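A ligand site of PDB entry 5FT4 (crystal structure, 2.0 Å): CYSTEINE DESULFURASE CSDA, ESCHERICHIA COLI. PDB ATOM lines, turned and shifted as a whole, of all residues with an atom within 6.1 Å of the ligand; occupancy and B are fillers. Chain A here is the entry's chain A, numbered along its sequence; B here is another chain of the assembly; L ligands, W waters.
The side-chain amino group of Lys 222 sits close to the side-chain amide nitrogen of Gln 199 (3.5 Å).
OG1 of Thr 90 is in hydrogen-bond range of OG of Ser 219 (2.6 Å).
The side-chain carboxylate of Asp 196 is in hydrogen-bond range of the backbone NH of Ala 198 (3.0 Å).
NE2 of His 221 sits at hydrogen-bond distance from OG1 of Thr 273 of chain B (3.4 Å).
The backbone carbonyl oxygen (O) of Ala 26 sits at hydrogen-bond distance from the side-chain amide nitrogen (NE2) of Gln 199 (3.0 Å).
ND1 of His 119 lies within hydrogen-bond range of N of Ala 121 (2.9 Å).
Thr 90 touches the ligand (N to O5, 3.7 Å).
CG of His 119 touches N1 of the ligand, at 3.3 Å.
Ala 121 touches the ligand (CB to C7, 3.6 Å).
Asn 171 touches the ligand (CB to O1, 3.6 Å).
Ala 198 touches the ligand.
Gly 272 of chain B touches the ligand (CA to O3, 3.7 Å).
Hydrophobic or aromatic side chains that line the ligand: His 119, Ala 121, Ala 198 and His 221.
13 residues have an atom within 4 Å of the ligand: Thr 90, Thr 91, His 119, Ala 121, Asn 171, Asp 196, Ala 198, Gln 199, Ser 219, His 221, Lys 222, Gly 272 of chain B and Thr 273 of chain B.
The nearest printed residue that does not touch the ligand is Gly 89 (4.1 Å).
A carbon (C5) of the ligand is covalently linked to the side-chain amino group (NZ) of Lys 222 (1.4 Å).
N of Thr 91 is in hydrogen-bond range of O5 of the ligand, 3.1 Å away.
The side-chain hydroxyl of Thr 91 is in hydrogen-bond range of an oxygen (O5) of the ligand (2.6 Å).
OG of Ser 219 sits at hydrogen-bond distance from O4 of the ligand.
The side-chain carboxylate of Asp 196 sits at hydrogen-bond distance from a nitrogen (N1) of the ligand, at 2.7 Å.
N of Thr 273 of chain B lies within hydrogen-bond range of O3 of the ligand (2.8 Å).
OG1 of Thr 273 of chain B is in hydrogen-bond range of O3 of the ligand, 2.7 Å away.
NE2 of Gln 199 sits at hydrogen-bond distance from O1 of the ligand, 2.9 Å away.
A ring nitrogen (NE2) of His 221 lies within hydrogen-bond range of an oxygen (O4) of the ligand (3.2 Å).
Water W1 bridges an oxygen (O4) of the ligand and the backbone carbonyl oxygen (O) of Arg 88.
Water W2 lies within hydrogen-bond range of O3 of the ligand (2.8 Å) and NZ of Lys 250 of chain B (3.2 Å).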
ATOM      1  N   ALA A  26     -16.516  28.103  14.956  1.00  0.00           N
ATOM      2  CA  ALA A  26     -16.022  28.748  16.185  1.00  0.00           C
ATOM      3  C   ALA A  26     -16.794  28.305  17.441  1.00  0.00           C
ATOM      4  O   ALA A  26     -16.229  28.303  18.545  1.00  0.00           O
ATOM      5  CB  ALA A  26     -16.064  30.292  16.042  1.00  0.00           C
ATOM      6  N   ALA A  27     -18.048  27.875  17.276  1.00  0.00           N
ATOM      7  CA  ALA A  27     -18.806  27.243  18.373  1.00  0.00           C
ATOM      8  C   ALA A  27     -18.414  25.757  18.518  1.00  0.00           C
ATOM      9  O   ALA A  27     -18.129  25.280  19.631  1.00  0.00           O
ATOM     10  CB  ALA A  27     -20.294  27.399  18.133  1.00  0.00           C
ATOM     11  N   ARG A  88     -11.548  18.406  30.772  1.00  0.00           N
ATOM     12  CA  ARG A  88     -12.770  18.178  30.005  1.00  0.00           C
ATOM     13  C   ARG A  88     -13.049  19.336  29.044  1.00  0.00           C
ATOM     14  O   ARG A  88     -14.007  19.273  28.273  1.00  0.00           O
ATOM     15  CB  ARG A  88     -13.954  17.919  30.943  1.00  0.00           C
ATOM     16  CG  ARG A  88     -14.460  19.049  31.732  1.00  0.00           C
ATOM     17  CD  ARG A  88     -15.714  18.590  32.468  1.00  0.00           C
ATOM     18  NE  ARG A  88     -16.398  19.658  33.172  1.00  0.00           N
ATOM     19  CZ  ARG A  88     -17.066  20.647  32.585  1.00  0.00           C
ATOM     20  NH1 ARG A  88     -17.147  20.708  31.262  1.00  0.00           N
ATOM     21  NH2 ARG A  88     -17.664  21.575  33.323  1.00  0.00           N
ATOM     22  N   GLY A  89     -12.183  20.353  29.102  1.00  0.00           N
ATOM     23  CA  GLY A  89     -12.340  21.567  28.325  1.00  0.00           C
ATOM     24  C   GLY A  89     -11.558  22.735  28.893  1.00  0.00           C
ATOM     25  O   GLY A  89     -11.055  22.714  30.032  1.00  0.00           O
ATOM     26  N   THR A  90     -11.454  23.758  28.050  1.00  0.00           N
ATOM     27  CA  THR A  90     -10.877  25.038  28.411  1.00  0.00           C
ATOM     28  C   THR A  90     -11.409  25.538  29.740  1.00  0.00           C
ATOM     29  O   THR A  90     -10.639  25.999  30.581  1.00  0.00           O
ATOM     30  CB  THR A  90     -11.185  26.100  27.310  1.00  0.00           C
ATOM     31  OG1 THR A  90     -10.672  25.644  26.060  1.00  0.00           O
ATOM     32  CG2 THR A  90     -10.596  27.443  27.619  1.00  0.00           C
ATOM     33  N   THR A  91     -12.719  25.413  29.938  1.00  0.00           N
ATOM     34  CA  THR A  91     -13.322  25.915  31.176  1.00  0.00           C
ATOM     35  C   THR A  91     -12.689  25.194  32.409  1.00  0.00           C
ATOM     36  O   THR A  91     -12.288  25.837  33.394  1.00  0.00           O
ATOM     37  CB  THR A  91     -14.853  25.754  31.136  1.00  0.00           C
ATOM     38  OG1 THR A  91     -15.389  26.384  29.960  1.00  0.00           O
ATOM     39  CG2 THR A  91     -15.548  26.330  32.410  1.00  0.00           C
ATOM     40  N   GLU A  92     -12.620  23.865  32.370  1.00  0.00           N
ATOM     41  CA  GLU A  92     -12.021  23.153  33.520  1.00  0.00           C
ATOM     42  C   GLU A  92     -10.586  23.560  33.705  1.00  0.00           C
ATOM     43  O   GLU A  92     -10.124  23.773  34.833  1.00  0.00           O
ATOM     44  CB  GLU A  92     -12.127  21.623  33.390  1.00  0.00           C
ATOM     45  CG  GLU A  92     -11.655  20.965  34.698  1.00  0.00           C
ATOM     46  CD  GLU A  92     -11.686  19.454  34.745  1.00  0.00           C
ATOM     47  OE1 GLU A  92     -11.676  18.772  33.682  1.00  0.00           O
ATOM     48  OE2 GLU A  92     -11.666  18.939  35.900  1.00  0.00           O
ATOM     49  N   ILE A  94      -9.093  26.324  33.110  1.00  0.00           N
ATOM     50  CA  ILE A  94      -8.902  27.627  33.713  1.00  0.00           C
ATOM     51  C   ILE A  94      -9.300  27.593  35.185  1.00  0.00           C
ATOM     52  O   ILE A  94      -8.602  28.119  36.032  1.00  0.00           O
ATOM     53  CB  ILE A  94      -9.697  28.700  32.948  1.00  0.00           C
ATOM     54  CG1 ILE A  94      -9.017  28.957  31.589  1.00  0.00           C
ATOM     55  CG2 ILE A  94      -9.712  29.980  33.733  1.00  0.00           C
ATOM     56  CD1 ILE A  94      -9.743  29.848  30.666  1.00  0.00           C
ATOM     57  N   HIS A 119     -13.857  35.600  27.217  1.00  0.00           N
ATOM     58  CA  HIS A 119     -14.941  34.632  27.333  1.00  0.00           C
ATOM     59  C   HIS A 119     -15.227  34.409  28.824  1.00  0.00           C
ATOM     60  O   HIS A 119     -14.315  34.459  29.668  1.00  0.00           O
ATOM     61  CB  HIS A 119     -14.501  33.329  26.628  1.00  0.00           C
ATOM     62  CG  HIS A 119     -15.556  32.259  26.513  1.00  0.00           C
ATOM     63  ND1 HIS A 119     -15.961  31.497  27.578  1.00  0.00           N
ATOM     64  CD2 HIS A 119     -16.214  31.772  25.425  1.00  0.00           C
ATOM     65  CE1 HIS A 119     -16.863  30.614  27.169  1.00  0.00           C
ATOM     66  NE2 HIS A 119     -17.028  30.768  25.871  1.00  0.00           N
ATOM     67  N   ALA A 121     -15.498  31.807  30.473  1.00  0.00           N
ATOM     68  CA  ALA A 121     -14.570  30.799  30.982  1.00  0.00           C
ATOM     69  C   ALA A 121     -13.337  31.419  31.625  1.00  0.00           C
ATOM     70  O   ALA A 121     -12.746  30.838  32.543  1.00  0.00           O
ATOM     71  CB  ALA A 121     -14.162  29.864  29.875  1.00  0.00           C
ATOM     72  N   ASN A 122     -12.899  32.572  31.126  1.00  0.00           N
ATOM     73  CA  ASN A 122     -11.699  33.213  31.665  1.00  0.00           C
ATOM     74  C   ASN A 122     -12.026  34.494  32.429  1.00  0.00           C
ATOM     75  O   ASN A 122     -11.197  35.419  32.535  1.00  0.00           O
ATOM     76  CB  ASN A 122     -10.691  33.470  30.540  1.00  0.00           C
ATOM     77  CG  ASN A 122      -9.272  33.606  31.061  1.00  0.00           C
ATOM     78  OD1 ASN A 122      -8.961  33.158  32.155  1.00  0.00           O
ATOM     79  ND2 ASN A 122      -8.392  34.212  30.280  1.00  0.00           N
ATOM     80  N   MET A 169      -7.076  34.967  21.643  1.00  0.00           N
ATOM     81  CA  MET A 169      -7.914  35.351  20.512  1.00  0.00           C
ATOM     82  C   MET A 169      -9.373  35.388  20.912  1.00  0.00           C
ATOM     83  O   MET A 169      -9.881  34.418  21.440  1.00  0.00           O
ATOM     84  CB  MET A 169      -7.711  34.383  19.356  1.00  0.00           C
ATOM     85  CG  MET A 169      -8.586  34.667  18.120  1.00  0.00           C
ATOM     86  SD  MET A 169      -8.378  33.356  16.869  1.00  0.00           S
ATOM     87  CE  MET A 169      -9.889  33.455  15.912  1.00  0.00           C
ATOM     88  N   SER A 170     -10.050  36.489  20.657  1.00  0.00           N
ATOM     89  CA  SER A 170     -11.467  36.586  21.023  1.00  0.00           C
ATOM     90  C   SER A 170     -12.368  35.746  20.128  1.00  0.00           C
ATOM     91  O   SER A 170     -12.191  35.711  18.905  1.00  0.00           O
ATOM     92  CB  SER A 170     -11.921  38.066  20.990  1.00  0.00           C
ATOM     93  OG  SER A 170     -13.328  38.189  20.942  1.00  0.00           O
ATOM     94  N   ASN A 171     -13.333  35.059  20.739  1.00  0.00           N
ATOM     95  CA  ASN A 171     -14.370  34.324  20.000  1.00  0.00           C
ATOM     96  C   ASN A 171     -15.458  35.220  19.404  1.00  0.00           C
ATOM     97  O   ASN A 171     -16.338  34.732  18.715  1.00  0.00           O
ATOM     98  CB  ASN A 171     -15.021  33.292  20.887  1.00  0.00           C
ATOM     99  CG  ASN A 171     -15.703  33.924  22.086  1.00  0.00           C
ATOM    100  OD1 ASN A 171     -15.133  34.776  22.739  1.00  0.00           O
ATOM    101  ND2 ASN A 171     -16.943  33.548  22.335  1.00  0.00           N
ATOM    102  N   ASP A 196      -6.065  32.068  27.595  1.00  0.00           N
ATOM    103  CA  ASP A 196      -7.163  31.323  27.023  1.00  0.00           C
ATOM    104  C   ASP A 196      -6.970  31.151  25.515  1.00  0.00           C
ATOM    105  O   ASP A 196      -7.176  32.087  24.738  1.00  0.00           O
ATOM    106  CB  ASP A 196      -8.478  32.054  27.310  1.00  0.00           C
ATOM    107  CG  ASP A 196      -9.718  31.328  26.734  1.00  0.00           C
ATOM    108  OD1 ASP A 196      -9.582  30.306  26.015  1.00  0.00           O
ATOM    109  OD2 ASP A 196     -10.838  31.817  27.010  1.00  0.00           O
ATOM    110  N   GLY A 197      -6.633  29.929  25.102  1.00  0.00           N
ATOM    111  CA  GLY A 197      -6.387  29.634  23.700  1.00  0.00           C
ATOM    112  C   GLY A 197      -7.482  28.818  23.009  1.00  0.00           C
ATOM    113  O   GLY A 197      -7.213  28.156  21.992  1.00  0.00           O
ATOM    114  N   ALA A 198      -8.705  28.862  23.506  1.00  0.00           N
ATOM    115  CA  ALA A 198      -9.762  28.035  22.907  1.00  0.00           C
ATOM    116  C   ALA A 198      -9.897  28.298  21.391  1.00  0.00           C
ATOM    117  O   ALA A 198     -10.118  27.376  20.593  1.00  0.00           O
ATOM    118  CB  ALA A 198     -11.078  28.311  23.579  1.00  0.00           C
ATOM    119  N   GLN A 199      -9.763  29.562  20.988  1.00  0.00           N
ATOM    120  CA  GLN A 199      -9.814  29.911  19.566  1.00  0.00           C
ATOM    121  C   GLN A 199      -8.397  29.943  18.985  1.00  0.00           C
ATOM    122  O   GLN A 199      -8.154  29.523  17.864  1.00  0.00           O
ATOM    123  CB  GLN A 199     -10.489  31.270  19.350  1.00  0.00           C
ATOM    124  CG  GLN A 199     -11.944  31.306  19.759  1.00  0.00           C
ATOM    125  CD  GLN A 199     -12.830  30.466  18.847  1.00  0.00           C
ATOM    126  OE1 GLN A 199     -12.532  30.269  17.663  1.00  0.00           O
ATOM    127  NE2 GLN A 199     -13.911  29.932  19.404  1.00  0.00           N
ATOM    128  N   SER A 219      -9.830  23.559  23.996  1.00  0.00           N
ATOM    129  CA  SER A 219     -10.845  22.531  23.945  1.00  0.00           C
ATOM    130  C   SER A 219     -10.765  21.702  22.671  1.00  0.00           C
ATOM    131  O   SER A 219     -10.603  22.240  21.585  1.00  0.00           O
ATOM    132  CB  SER A 219     -12.241  23.181  24.072  1.00  0.00           C
ATOM    133  OG  SER A 219     -12.399  23.803  25.354  1.00  0.00           O
ATOM    134  N   GLY A 220     -10.900  20.390  22.818  1.00  0.00           N
ATOM    135  CA  GLY A 220     -10.811  19.487  21.696  1.00  0.00           C
ATOM    136  C   GLY A 220     -11.895  19.628  20.641  1.00  0.00           C
ATOM    137  O   GLY A 220     -11.625  19.475  19.441  1.00  0.00           O
ATOM    138  N   HIS A 221     -13.107  19.959  21.068  1.00  0.00           N
ATOM    139  CA  HIS A 221     -14.265  19.880  20.160  1.00  0.00           C
ATOM    140  C   HIS A 221     -14.218  21.032  19.149  1.00  0.00           C
ATOM    141  O   HIS A 221     -14.853  20.974  18.089  1.00  0.00           O
ATOM    142  CB  HIS A 221     -15.590  19.874  20.957  1.00  0.00           C
ATOM    143  CG  HIS A 221     -15.925  21.196  21.598  1.00  0.00           C
ATOM    144  ND1 HIS A 221     -16.697  22.155  20.974  1.00  0.00           N
ATOM    145  CD2 HIS A 221     -15.630  21.694  22.829  1.00  0.00           C
ATOM    146  CE1 HIS A 221     -16.841  23.200  21.775  1.00  0.00           C
ATOM    147  NE2 HIS A 221     -16.195  22.950  22.904  1.00  0.00           N
ATOM    148  N   LYS A 222     -13.456  22.082  19.472  1.00  0.00           N
ATOM    149  CA  LYS A 222     -13.241  23.216  18.551  1.00  0.00           C
ATOM    150  C   LYS A 222     -12.112  22.864  17.622  1.00  0.00           C
ATOM    151  O   LYS A 222     -12.058  23.398  16.537  1.00  0.00           O
ATOM    152  CB  LYS A 222     -12.954  24.522  19.278  1.00  0.00           C
ATOM    153  CG  LYS A 222     -14.261  25.155  19.769  1.00  0.00           C
ATOM    154  CD  LYS A 222     -13.994  26.220  20.847  1.00  0.00           C
ATOM    155  CE  LYS A 222     -15.378  26.751  21.293  1.00  0.00           C
ATOM    156  NZ  LYS A 222     -15.240  28.028  22.003  1.00  0.00           N
ATOM    157  N   ILE A 229     -13.243  16.697  26.130  1.00  0.00           N
ATOM    158  CA  ILE A 229     -11.794  16.674  26.271  1.00  0.00           C
ATOM    159  C   ILE A 229     -11.161  18.065  26.011  1.00  0.00           C
ATOM    160  O   ILE A 229     -11.522  18.774  25.066  1.00  0.00           O
ATOM    161  CB  ILE A 229     -11.139  15.600  25.317  1.00  0.00           C
ATOM    162  CG1 ILE A 229      -9.655  15.364  25.680  1.00  0.00           C
ATOM    163  CG2 ILE A 229     -11.292  15.979  23.854  1.00  0.00           C
ATOM    164  CD1 ILE A 229      -9.480  14.638  27.062  1.00  0.00           C
ATOM    165  N   LYS B 250     -22.476  28.844  30.287  1.00  0.00           N
ATOM    166  CA  LYS B 250     -23.551  27.884  30.422  1.00  0.00           C
ATOM    167  C   LYS B 250     -24.077  27.802  31.855  1.00  0.00           C
ATOM    168  O   LYS B 250     -25.283  27.792  32.034  1.00  0.00           O
ATOM    169  CB  LYS B 250     -23.148  26.495  29.919  1.00  0.00           C
ATOM    170  CG  LYS B 250     -22.282  26.503  28.629  1.00  0.00           C
ATOM    171  CD  LYS B 250     -22.932  27.189  27.464  1.00  0.00           C
ATOM    172  CE  LYS B 250     -21.904  27.511  26.382  1.00  0.00           C
ATOM    173  NZ  LYS B 250     -21.278  26.295  25.805  1.00  0.00           N
ATOM    174  N   ALA B 271     -20.591  23.868  34.172  1.00  0.00           N
ATOM    175  CA  ALA B 271     -19.983  24.955  33.386  1.00  0.00           C
ATOM    176  C   ALA B 271     -19.496  24.409  32.029  1.00  0.00           C
ATOM    177  O   ALA B 271     -19.111  23.257  31.931  1.00  0.00           O
ATOM    178  CB  ALA B 271     -18.825  25.583  34.106  1.00  0.00           C
ATOM    179  N   GLY B 272     -19.533  25.237  30.993  1.00  0.00           N
ATOM    180  CA  GLY B 272     -18.847  24.889  29.760  1.00  0.00           C
ATOM    181  C   GLY B 272     -19.667  23.974  28.855  1.00  0.00           C
ATOM    182  O   GLY B 272     -20.734  23.477  29.214  1.00  0.00           O
ATOM    183  N   THR B 273     -19.121  23.742  27.671  1.00  0.00           N
ATOM    184  CA  THR B 273     -19.697  22.795  26.726  1.00  0.00           C
ATOM    185  C   THR B 273     -19.759  21.416  27.358  1.00  0.00           C
ATOM    186  O   THR B 273     -18.758  20.919  27.829  1.00  0.00           O
ATOM    187  CB  THR B 273     -18.857  22.695  25.434  1.00  0.00           C
ATOM    188  OG1 THR B 273     -18.768  23.988  24.846  1.00  0.00           O
ATOM    189  CG2 THR B 273     -19.488  21.705  24.441  1.00  0.00           C
ATOM    190  N   PRO B 274     -20.955  20.807  27.366  1.00  0.00           N
ATOM    191  CA  PRO B 274     -21.089  19.443  27.877  1.00  0.00           C
ATOM    192  C   PRO B 274     -20.357  18.415  27.027  1.00  0.00           C
ATOM    193  O   PRO B 274     -19.990  18.656  25.853  1.00  0.00           O
ATOM    194  CB  PRO B 274     -22.613  19.190  27.834  1.00  0.00           C
ATOM    195  CG  PRO B 274     -23.248  20.477  27.616  1.00  0.00           C
ATOM    196  CD  PRO B 274     -22.253  21.367  26.961  1.00  0.00           C
HETATM  197  N1  LIG L   1     -12.876  30.558  25.737  1.00  0.00           N
HETATM  198  C1  LIG L   1     -13.057  30.814  24.447  1.00  0.00           C
HETATM  199  C2  LIG L   1     -12.367  32.081  23.843  1.00  0.00           C
HETATM  200  C3  LIG L   1     -13.856  29.927  23.667  1.00  0.00           C
HETATM  201  O1  LIG L   1     -14.029  30.177  22.317  1.00  0.00           O
HETATM  202  C4  LIG L   1     -14.453  28.817  24.249  1.00  0.00           C
HETATM  203  C5  LIG L   1     -15.346  27.801  23.407  1.00  0.00           C
HETATM  204  C6  LIG L   1     -14.269  28.559  25.571  1.00  0.00           C
HETATM  205  C7  LIG L   1     -13.482  29.449  26.324  1.00  0.00           C
HETATM  206  C8  LIG L   1     -14.946  27.348  26.329  1.00  0.00           C
HETATM  207  O2  LIG L   1     -14.696  26.032  25.898  1.00  0.00           O
HETATM  208  P1  LIG L   1     -15.444  24.814  26.565  1.00  0.00           P
HETATM  209  O3  LIG L   1     -16.946  25.102  26.542  1.00  0.00           O
HETATM  210  O4  LIG L   1     -15.044  23.600  25.789  1.00  0.00           O
HETATM  211  O5  LIG L   1     -15.027  24.741  28.017  1.00  0.00           O
HETATM  212  O   HOH W   1     -15.032  20.925  26.111  1.00  0.00           O
HETATM  213  O   HOH W   2     -18.602  27.239  27.220  1.00  0.00           O
